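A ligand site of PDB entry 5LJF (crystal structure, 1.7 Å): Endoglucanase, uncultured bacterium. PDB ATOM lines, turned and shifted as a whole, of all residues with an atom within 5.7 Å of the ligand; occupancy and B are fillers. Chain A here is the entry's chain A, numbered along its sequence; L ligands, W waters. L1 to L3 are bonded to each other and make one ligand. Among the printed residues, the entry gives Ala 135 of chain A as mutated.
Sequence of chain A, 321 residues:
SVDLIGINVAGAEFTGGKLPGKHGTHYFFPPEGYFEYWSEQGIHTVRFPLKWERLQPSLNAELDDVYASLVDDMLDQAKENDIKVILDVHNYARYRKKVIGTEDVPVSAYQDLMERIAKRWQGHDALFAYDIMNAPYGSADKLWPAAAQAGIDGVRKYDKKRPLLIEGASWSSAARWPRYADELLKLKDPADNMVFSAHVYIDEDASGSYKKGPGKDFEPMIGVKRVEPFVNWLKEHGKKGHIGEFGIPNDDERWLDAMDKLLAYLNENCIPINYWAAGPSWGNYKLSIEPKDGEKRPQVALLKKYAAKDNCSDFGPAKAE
The backbone carbonyl oxygen of Asn 134 sits at hydrogen-bond distance from the backbone NH of Tyr 92 (2.8 Å). A ring nitrogen (NE2) of His 90 is in hydrogen-bond range of the side-chain amide nitrogen (ND2) of Asn 134. The side-chain amide oxygen (OD1) of Asn 134 lies within hydrogen-bond range of the guanidinium group (NH2) of Arg 47. The side-chain amide oxygen (OD1) of Asn 134 sits close to the side-chain carboxylate (OE2) of Glu 245, at 3.2 Å. OE1 of Glu 245 is in hydrogen-bond range of OH of Tyr 201 (2.7 Å). OG of Ser 170 sits at hydrogen-bond distance from NH2 of Arg 176, 2.8 Å away. The side-chain carboxylate of Glu 245 lies within salt-bridge range of the guanidinium group of Arg 47 (3.1 Å). The side-chain hydroxyl (OG) of Ser 207 is in hydrogen-bond range of the side-chain carboxylate (OD1) of Asp 205.
The side-chain carboxylate (OE2) of Glu 245 is in hydrogen-bond range of an oxygen (O2) of LG3 L3. ND2 of Asn 134 lies within hydrogen-bond range of O2 of LG3 L3, at 3.0 Å. The backbone carbonyl oxygen (O) of Asp 205 sits at hydrogen-bond distance from an oxygen (O2) of LIG L1 (2.6 Å). A ring nitrogen (NE2) of His 90 is in hydrogen-bond range of an oxygen (O2) of LG3 L3, at 2.8 Å. O2 of LIG L1 sits at hydrogen-bond distance from NH1 of Arg 176 (3.0 Å). The backbone carbonyl oxygen (O) of Ala 206 is in hydrogen-bond range of an oxygen (O5) of LG2 L2, 2.7 Å away.
Water W5 lies within hydrogen-bond range of an oxygen (O1) of LG3 L3 (2.5 Å), a ring nitrogen (ND1) of His 199 (2.7 Å) and the backbone carbonyl oxygen (O) of Trp 171 (2.9 Å). Water W2 lies within hydrogen-bond range of an oxygen (O5) of LG2 L2 (2.7 Å) and the backbone carbonyl oxygen of Trp 171 (2.9 Å). Water W6 bridges an oxygen (O3) of LIG L1 (2.7 Å) and the guanidinium group of Arg 176 (2.9 Å). Water W7 bridges OE2 of Glu 13 (2.6 Å) and O3 of LG3 L3 (2.8 Å). Water W1 lies within hydrogen-bond range of NE1 of Trp 276 (3.0 Å) and O3 of LG3 L3 (3.0 Å). Water W4 lies within hydrogen-bond range of N of Tyr 201 (3.0 Å), O of Ala 206 (3.1 Å) and O5 of LG2 L2 (3.5 Å).
Residues that only touch the ligand: Tyr 92 (3.1 Å), Trp 276 (3.2 Å), Ser 207 (3.3 Å), Tyr 201 (3.7 Å), Trp 171 (3.7 Å) and His 199 (3.9 Å). Hydrophobic or aromatic side chains that line the ligand: His 90, Trp 171, Tyr 201, Ala 206 and Trp 276. 12 residues have an atom within 4 Å of the ligand: His 90, Tyr 92, Asn 134, Trp 171, Arg 176, His 199, Tyr 201, Asp 205, Ala 206, Ser 207, Glu 245 and Trp 276. The nearest printed residue that does not touch the ligand is Ala 135 (4.3 Å).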
ATOM      1  N   GLU A  13      -6.016  18.753 -15.315  1.00  0.00           N
ATOM      2  CA  GLU A  13      -6.591  19.278 -16.536  1.00  0.00           C
ATOM      3  C   GLU A  13      -6.125  18.501 -17.774  1.00  0.00           C
ATOM      4  O   GLU A  13      -6.518  18.845 -18.892  1.00  0.00           O
ATOM      5  CB  GLU A  13      -6.242  20.788 -16.666  1.00  0.00           C
ATOM      6  CG  GLU A  13      -4.869  21.108 -17.244  1.00  0.00           C
ATOM      7  CD  GLU A  13      -3.659  20.776 -16.367  1.00  0.00           C
ATOM      8  OE1 GLU A  13      -3.784  20.139 -15.296  1.00  0.00           O
ATOM      9  OE2 GLU A  13      -2.537  21.169 -16.776  1.00  0.00           O
ATOM     10  N   ARG A  47      -0.020  26.686  -7.650  1.00  0.00           N
ATOM     11  CA  ARG A  47      -1.125  26.973  -8.555  1.00  0.00           C
ATOM     12  C   ARG A  47      -1.594  25.641  -9.111  1.00  0.00           C
ATOM     13  O   ARG A  47      -0.782  24.841  -9.574  1.00  0.00           O
ATOM     14  CB  ARG A  47      -0.680  27.897  -9.691  1.00  0.00           C
ATOM     15  CG  ARG A  47      -1.769  28.254 -10.681  1.00  0.00           C
ATOM     16  CD  ARG A  47      -1.177  29.304 -11.620  1.00  0.00           C
ATOM     17  NE  ARG A  47      -2.095  29.785 -12.634  1.00  0.00           N
ATOM     18  CZ  ARG A  47      -2.126  29.361 -13.890  1.00  0.00           C
ATOM     19  NH1 ARG A  47      -1.331  28.387 -14.313  1.00  0.00           N
ATOM     20  NH2 ARG A  47      -2.973  29.922 -14.753  1.00  0.00           N
ATOM     21  N   HIS A  90      -8.692  26.230 -15.665  1.00  0.00           N
ATOM     22  CA  HIS A  90      -7.635  26.200 -16.677  1.00  0.00           C
ATOM     23  C   HIS A  90      -8.245  26.040 -18.072  1.00  0.00           C
ATOM     24  O   HIS A  90      -8.015  25.050 -18.766  1.00  0.00           O
ATOM     25  CB  HIS A  90      -6.644  25.081 -16.366  1.00  0.00           C
ATOM     26  CG  HIS A  90      -5.282  25.277 -16.967  1.00  0.00           C
ATOM     27  ND1 HIS A  90      -4.309  26.044 -16.368  1.00  0.00           N
ATOM     28  CD2 HIS A  90      -4.729  24.795 -18.114  1.00  0.00           C
ATOM     29  CE1 HIS A  90      -3.207  25.999 -17.099  1.00  0.00           C
ATOM     30  NE2 HIS A  90      -3.450  25.273 -18.179  1.00  0.00           N
ATOM     31  N   TYR A  92      -9.015  28.763 -20.797  1.00  0.00           N
ATOM     32  CA  TYR A  92      -8.831  29.583 -21.993  1.00  0.00           C
ATOM     33  C   TYR A  92     -10.096  30.361 -22.360  1.00  0.00           C
ATOM     34  O   TYR A  92     -10.325  30.661 -23.532  1.00  0.00           O
ATOM     35  CB  TYR A  92      -8.378  28.703 -23.185  1.00  0.00           C
ATOM     36  CG  TYR A  92      -7.264  27.781 -22.785  1.00  0.00           C
ATOM     37  CD1 TYR A  92      -5.965  28.232 -22.733  1.00  0.00           C
ATOM     38  CD2 TYR A  92      -7.523  26.470 -22.412  1.00  0.00           C
ATOM     39  CE1 TYR A  92      -4.925  27.381 -22.351  1.00  0.00           C
ATOM     40  CE2 TYR A  92      -6.515  25.620 -22.003  1.00  0.00           C
ATOM     41  CZ  TYR A  92      -5.216  26.082 -21.980  1.00  0.00           C
ATOM     42  OH  TYR A  92      -4.207  25.237 -21.592  1.00  0.00           O
ATOM     43  N   ASN A 134      -7.523  30.608 -16.894  1.00  0.00           N
ATOM     44  CA  ASN A 134      -6.190  30.512 -17.470  1.00  0.00           C
ATOM     45  C   ASN A 134      -6.202  30.951 -18.936  1.00  0.00           C
ATOM     46  O   ASN A 134      -7.020  30.459 -19.717  1.00  0.00           O
ATOM     47  CB  ASN A 134      -5.691  29.074 -17.381  1.00  0.00           C
ATOM     48  CG  ASN A 134      -4.350  28.905 -18.041  1.00  0.00           C
ATOM     49  OD1 ASN A 134      -3.373  29.517 -17.617  1.00  0.00           O
ATOM     50  ND2 ASN A 134      -4.296  28.085 -19.079  1.00  0.00           N
ATOM     51  N   ALA A 135      -5.301  31.870 -19.275  1.00  0.00           N
ATOM     52  CA  ALA A 135      -4.882  32.145 -20.645  1.00  0.00           C
ATOM     53  C   ALA A 135      -6.033  32.261 -21.646  1.00  0.00           C
ATOM     54  O   ALA A 135      -6.113  31.476 -22.600  1.00  0.00           O
ATOM     55  CB  ALA A 135      -3.888  31.074 -21.102  1.00  0.00           C
ATOM     56  N   SER A 170      -4.682  37.209 -24.998  1.00  0.00           N
ATOM     57  CA  SER A 170      -3.499  36.771 -25.725  1.00  0.00           C
ATOM     58  C   SER A 170      -2.645  35.848 -24.857  1.00  0.00           C
ATOM     59  O   SER A 170      -1.452  36.058 -24.659  1.00  0.00           O
ATOM     60  CB  SER A 170      -2.710  38.002 -26.209  1.00  0.00           C
ATOM     61  OG  SER A 170      -1.741  37.669 -27.189  1.00  0.00           O
ATOM     62  N   TRP A 171      -3.280  34.805 -24.332  1.00  0.00           N
ATOM     63  CA  TRP A 171      -2.622  33.826 -23.449  1.00  0.00           C
ATOM     64  C   TRP A 171      -2.008  34.503 -22.218  1.00  0.00           C
ATOM     65  O   TRP A 171      -1.001  34.045 -21.688  1.00  0.00           O
ATOM     66  CB  TRP A 171      -1.570  32.991 -24.193  1.00  0.00           C
ATOM     67  CG  TRP A 171      -2.079  32.239 -25.399  1.00  0.00           C
ATOM     68  CD1 TRP A 171      -2.647  30.996 -25.419  1.00  0.00           C
ATOM     69  CD2 TRP A 171      -2.065  32.699 -26.759  1.00  0.00           C
ATOM     70  NE1 TRP A 171      -2.974  30.647 -26.707  1.00  0.00           N
ATOM     71  CE2 TRP A 171      -2.633  31.675 -27.552  1.00  0.00           C
ATOM     72  CE3 TRP A 171      -1.608  33.854 -27.380  1.00  0.00           C
ATOM     73  CZ2 TRP A 171      -2.763  31.794 -28.935  1.00  0.00           C
ATOM     74  CZ3 TRP A 171      -1.748  33.972 -28.763  1.00  0.00           C
ATOM     75  CH2 TRP A 171      -2.326  32.944 -29.520  1.00  0.00           C
ATOM     76  N   ARG A 176       2.972  41.330 -24.140  1.00  0.00           N
ATOM     77  CA  ARG A 176       1.986  42.108 -24.875  1.00  0.00           C
ATOM     78  C   ARG A 176       0.957  42.723 -23.950  1.00  0.00           C
ATOM     79  O   ARG A 176      -0.011  43.311 -24.428  1.00  0.00           O
ATOM     80  CB  ARG A 176       1.302  41.238 -25.938  1.00  0.00           C
ATOM     81  CG  ARG A 176       2.258  40.708 -27.011  1.00  0.00           C
ATOM     82  CD  ARG A 176       1.529  39.918 -28.097  1.00  0.00           C
ATOM     83  NE  ARG A 176       0.878  38.700 -27.596  1.00  0.00           N
ATOM     84  CZ  ARG A 176       1.494  37.531 -27.412  1.00  0.00           C
ATOM     85  NH1 ARG A 176       2.802  37.420 -27.667  1.00  0.00           N
ATOM     86  NH2 ARG A 176       0.822  36.477 -26.959  1.00  0.00           N
ATOM     87  N   HIS A 199       1.704  35.682 -17.947  1.00  0.00           N
ATOM     88  CA  HIS A 199       2.531  34.509 -18.197  1.00  0.00           C
ATOM     89  C   HIS A 199       3.706  34.878 -19.100  1.00  0.00           C
ATOM     90  O   HIS A 199       3.615  35.776 -19.929  1.00  0.00           O
ATOM     91  CB  HIS A 199       1.735  33.412 -18.860  1.00  0.00           C
ATOM     92  CG  HIS A 199       0.603  32.894 -18.039  1.00  0.00           C
ATOM     93  ND1 HIS A 199      -0.300  31.980 -18.526  1.00  0.00           N
ATOM     94  CD2 HIS A 199       0.225  33.161 -16.763  1.00  0.00           C
ATOM     95  CE1 HIS A 199      -1.192  31.706 -17.597  1.00  0.00           C
ATOM     96  NE2 HIS A 199      -0.897  32.407 -16.513  1.00  0.00           N
ATOM     97  N   TYR A 201       6.979  32.934 -21.299  1.00  0.00           N
ATOM     98  CA  TYR A 201       7.889  31.914 -21.763  1.00  0.00           C
ATOM     99  C   TYR A 201       8.930  32.589 -22.647  1.00  0.00           C
ATOM    100  O   TYR A 201       8.653  33.635 -23.249  1.00  0.00           O
ATOM    101  CB  TYR A 201       7.156  30.821 -22.553  1.00  0.00           C
ATOM    102  CG  TYR A 201       6.224  30.038 -21.682  1.00  0.00           C
ATOM    103  CD1 TYR A 201       6.689  28.976 -20.909  1.00  0.00           C
ATOM    104  CD2 TYR A 201       4.881  30.386 -21.583  1.00  0.00           C
ATOM    105  CE1 TYR A 201       5.844  28.256 -20.107  1.00  0.00           C
ATOM    106  CE2 TYR A 201       4.015  29.680 -20.768  1.00  0.00           C
ATOM    107  CZ  TYR A 201       4.502  28.608 -20.029  1.00  0.00           C
ATOM    108  OH  TYR A 201       3.677  27.876 -19.225  1.00  0.00           O
ATOM    109  N   ASP A 205       8.827  32.539 -29.870  1.00  0.00           N
ATOM    110  CA  ASP A 205       7.419  32.887 -30.036  1.00  0.00           C
ATOM    111  C   ASP A 205       6.658  32.897 -28.707  1.00  0.00           C
ATOM    112  O   ASP A 205       5.435  33.027 -28.722  1.00  0.00           O
ATOM    113  CB  ASP A 205       6.750  31.945 -31.054  1.00  0.00           C
ATOM    114  CG  ASP A 205       6.535  30.539 -30.541  1.00  0.00           C
ATOM    115  OD1 ASP A 205       7.009  30.200 -29.435  1.00  0.00           O
ATOM    116  OD2 ASP A 205       5.889  29.740 -31.254  1.00  0.00           O
ATOM    117  N   ALA A 206       7.357  32.755 -27.581  1.00  0.00           N
ATOM    118  CA  ALA A 206       6.782  32.816 -26.232  1.00  0.00           C
ATOM    119  C   ALA A 206       5.683  31.776 -26.006  1.00  0.00           C
ATOM    120  O   ALA A 206       4.851  31.905 -25.091  1.00  0.00           O
ATOM    121  CB  ALA A 206       6.247  34.231 -25.928  1.00  0.00           C
ATOM    122  N   SER A 207       5.680  30.714 -26.813  1.00  0.00           N
ATOM    123  CA  SER A 207       4.703  29.657 -26.632  1.00  0.00           C
ATOM    124  C   SER A 207       5.075  28.682 -25.530  1.00  0.00           C
ATOM    125  O   SER A 207       4.210  27.927 -25.087  1.00  0.00           O
ATOM    126  CB  SER A 207       4.519  28.874 -27.938  1.00  0.00           C
ATOM    127  OG  SER A 207       5.713  28.164 -28.243  1.00  0.00           O
ATOM    128  N   GLY A 208       6.329  28.682 -25.080  1.00  0.00           N
ATOM    129  CA  GLY A 208       6.730  27.639 -24.161  1.00  0.00           C
ATOM    130  C   GLY A 208       6.936  26.289 -24.809  1.00  0.00           C
ATOM    131  O   GLY A 208       7.106  25.298 -24.096  1.00  0.00           O
ATOM    132  N   GLU A 245       2.674  31.682 -14.839  1.00  0.00           N
ATOM    133  CA  GLU A 245       3.380  30.644 -15.578  1.00  0.00           C
ATOM    134  C   GLU A 245       4.705  31.174 -16.103  1.00  0.00           C
ATOM    135  O   GLU A 245       4.756  32.258 -16.713  1.00  0.00           O
ATOM    136  CB  GLU A 245       2.563  30.101 -16.758  1.00  0.00           C
ATOM    137  CG  GLU A 245       1.302  29.420 -16.343  1.00  0.00           C
ATOM    138  CD  GLU A 245       0.606  28.740 -17.484  1.00  0.00           C
ATOM    139  OE1 GLU A 245       1.173  28.724 -18.618  1.00  0.00           O
ATOM    140  OE2 GLU A 245      -0.514  28.234 -17.254  1.00  0.00           O
ATOM    141  N   TRP A 276       6.122  26.894 -14.181  1.00  0.00           N
ATOM    142  CA  TRP A 276       5.402  25.890 -14.952  1.00  0.00           C
ATOM    143  C   TRP A 276       6.366  24.838 -15.482  1.00  0.00           C
ATOM    144  O   TRP A 276       7.123  25.156 -16.371  1.00  0.00           O
ATOM    145  CB  TRP A 276       4.690  26.499 -16.166  1.00  0.00           C
ATOM    146  CG  TRP A 276       3.872  25.451 -16.892  1.00  0.00           C
ATOM    147  CD1 TRP A 276       4.296  24.644 -17.921  1.00  0.00           C
ATOM    148  CD2 TRP A 276       2.520  25.083 -16.621  1.00  0.00           C
ATOM    149  NE1 TRP A 276       3.275  23.792 -18.291  1.00  0.00           N
ATOM    150  CE2 TRP A 276       2.176  24.043 -17.511  1.00  0.00           C
ATOM    151  CE3 TRP A 276       1.554  25.522 -15.709  1.00  0.00           C
ATOM    152  CZ2 TRP A 276       0.918  23.443 -17.518  1.00  0.00           C
ATOM    153  CZ3 TRP A 276       0.315  24.932 -15.708  1.00  0.00           C
ATOM    154  CH2 TRP A 276       0.001  23.906 -16.614  1.00  0.00           C
HETATM  155  C1  LIG L   1       2.257  33.844 -28.894  1.00  0.00           C
HETATM  156  C2  LIG L   1       2.216  32.464 -28.200  1.00  0.00           C
HETATM  157  C3  LIG L   1       1.147  31.541 -28.855  1.00  0.00           C
HETATM  158  C4  LIG L   1       1.347  31.574 -30.383  1.00  0.00           C
HETATM  159  C5  LIG L   1       0.252  30.743 -31.092  1.00  0.00           C
HETATM  160  C6  LIG L   1       2.465  33.637 -30.409  1.00  0.00           C
HETATM  161  O1  LIG L   1       2.261  34.905 -30.990  1.00  0.00           O
HETATM  162  O2  LIG L   1       3.305  34.545 -28.300  1.00  0.00           O
HETATM  163  O3  LIG L   1       1.871  32.673 -26.831  1.00  0.00           O
HETATM  164  O4  LIG L   1       1.334  30.261 -28.372  1.00  0.00           O
HETATM  165  O5  LIG L   1       1.400  32.876 -30.897  1.00  0.00           O
HETATM  166  O6  LIG L   1       0.686  30.535 -32.387  1.00  0.00           O
HETATM  167  C1  LG2 L   2       0.392  28.347 -27.276  1.00  0.00           C
HETATM  168  C2  LG2 L   2      -0.339  27.964 -25.967  1.00  0.00           C
HETATM  169  C3  LG2 L   2       0.484  28.403 -24.703  1.00  0.00           C
HETATM  170  C4  LG2 L   2       0.937  29.892 -24.891  1.00  0.00           C
HETATM  171  C5  LG2 L   2       2.036  30.324 -23.874  1.00  0.00           C
HETATM  172  C6  LG2 L   2       0.599  29.853 -27.274  1.00  0.00           C
HETATM  173  O1  LG2 L   2      -0.464  28.041 -28.342  1.00  0.00           O
HETATM  174  O2  LG2 L   2      -0.435  26.589 -25.944  1.00  0.00           O
HETATM  175  O3  LG2 L   2      -0.370  28.244 -23.607  1.00  0.00           O
HETATM  176  O4  LG2 L   2       1.456  30.148 -26.178  1.00  0.00           O
HETATM  177  O5  LG2 L   2       2.350  31.653 -24.056  1.00  0.00           O
HETATM  178  C1  LG3 L   3      -0.798  27.709 -21.382  1.00  0.00           C
HETATM  179  C2  LG3 L   3      -0.685  26.598 -20.365  1.00  0.00           C
HETATM  180  C3  LG3 L   3      -1.224  25.265 -20.945  1.00  0.00           C
HETATM  181  C4  LG3 L   3      -0.503  24.999 -22.310  1.00  0.00           C
HETATM  182  C5  LG3 L   3      -1.086  23.768 -23.037  1.00  0.00           C
HETATM  183  C6  LG3 L   3      -0.057  27.294 -22.688  1.00  0.00           C
HETATM  184  O1  LG3 L   3      -0.215  28.874 -20.861  1.00  0.00           O
HETATM  185  O2  LG3 L   3      -1.520  26.991 -19.316  1.00  0.00           O
HETATM  186  O3  LG3 L   3      -0.889  24.300 -20.051  1.00  0.00           O
HETATM  187  O4  LG3 L   3      -0.649  26.112 -23.157  1.00  0.00           O
HETATM  188  O5  LG3 L   3      -0.767  23.916 -24.389  1.00  0.00           O
HETATM  189  O   HOH W   1       1.782  23.007 -20.725  1.00  0.00           O
HETATM  190  O   HOH W   2       1.721  33.897 -22.744  1.00  0.00           O
HETATM  191  O   HOH W   3       4.845  36.436 -30.614  1.00  0.00           O
HETATM  192  O   HOH W   4       4.606  33.959 -22.808  1.00  0.00           O
HETATM  193  O   HOH W   5       0.081  31.391 -21.133  1.00  0.00           O
HETATM  194  O   HOH W   6       2.498  34.829 -25.345  1.00  0.00           O
HETATM  195  O   HOH W   7      -2.292  21.952 -19.269  1.00  0.00           O
HETATM  196  O   HOH W   8      -3.429  28.148 -28.001  1.00  0.00           O
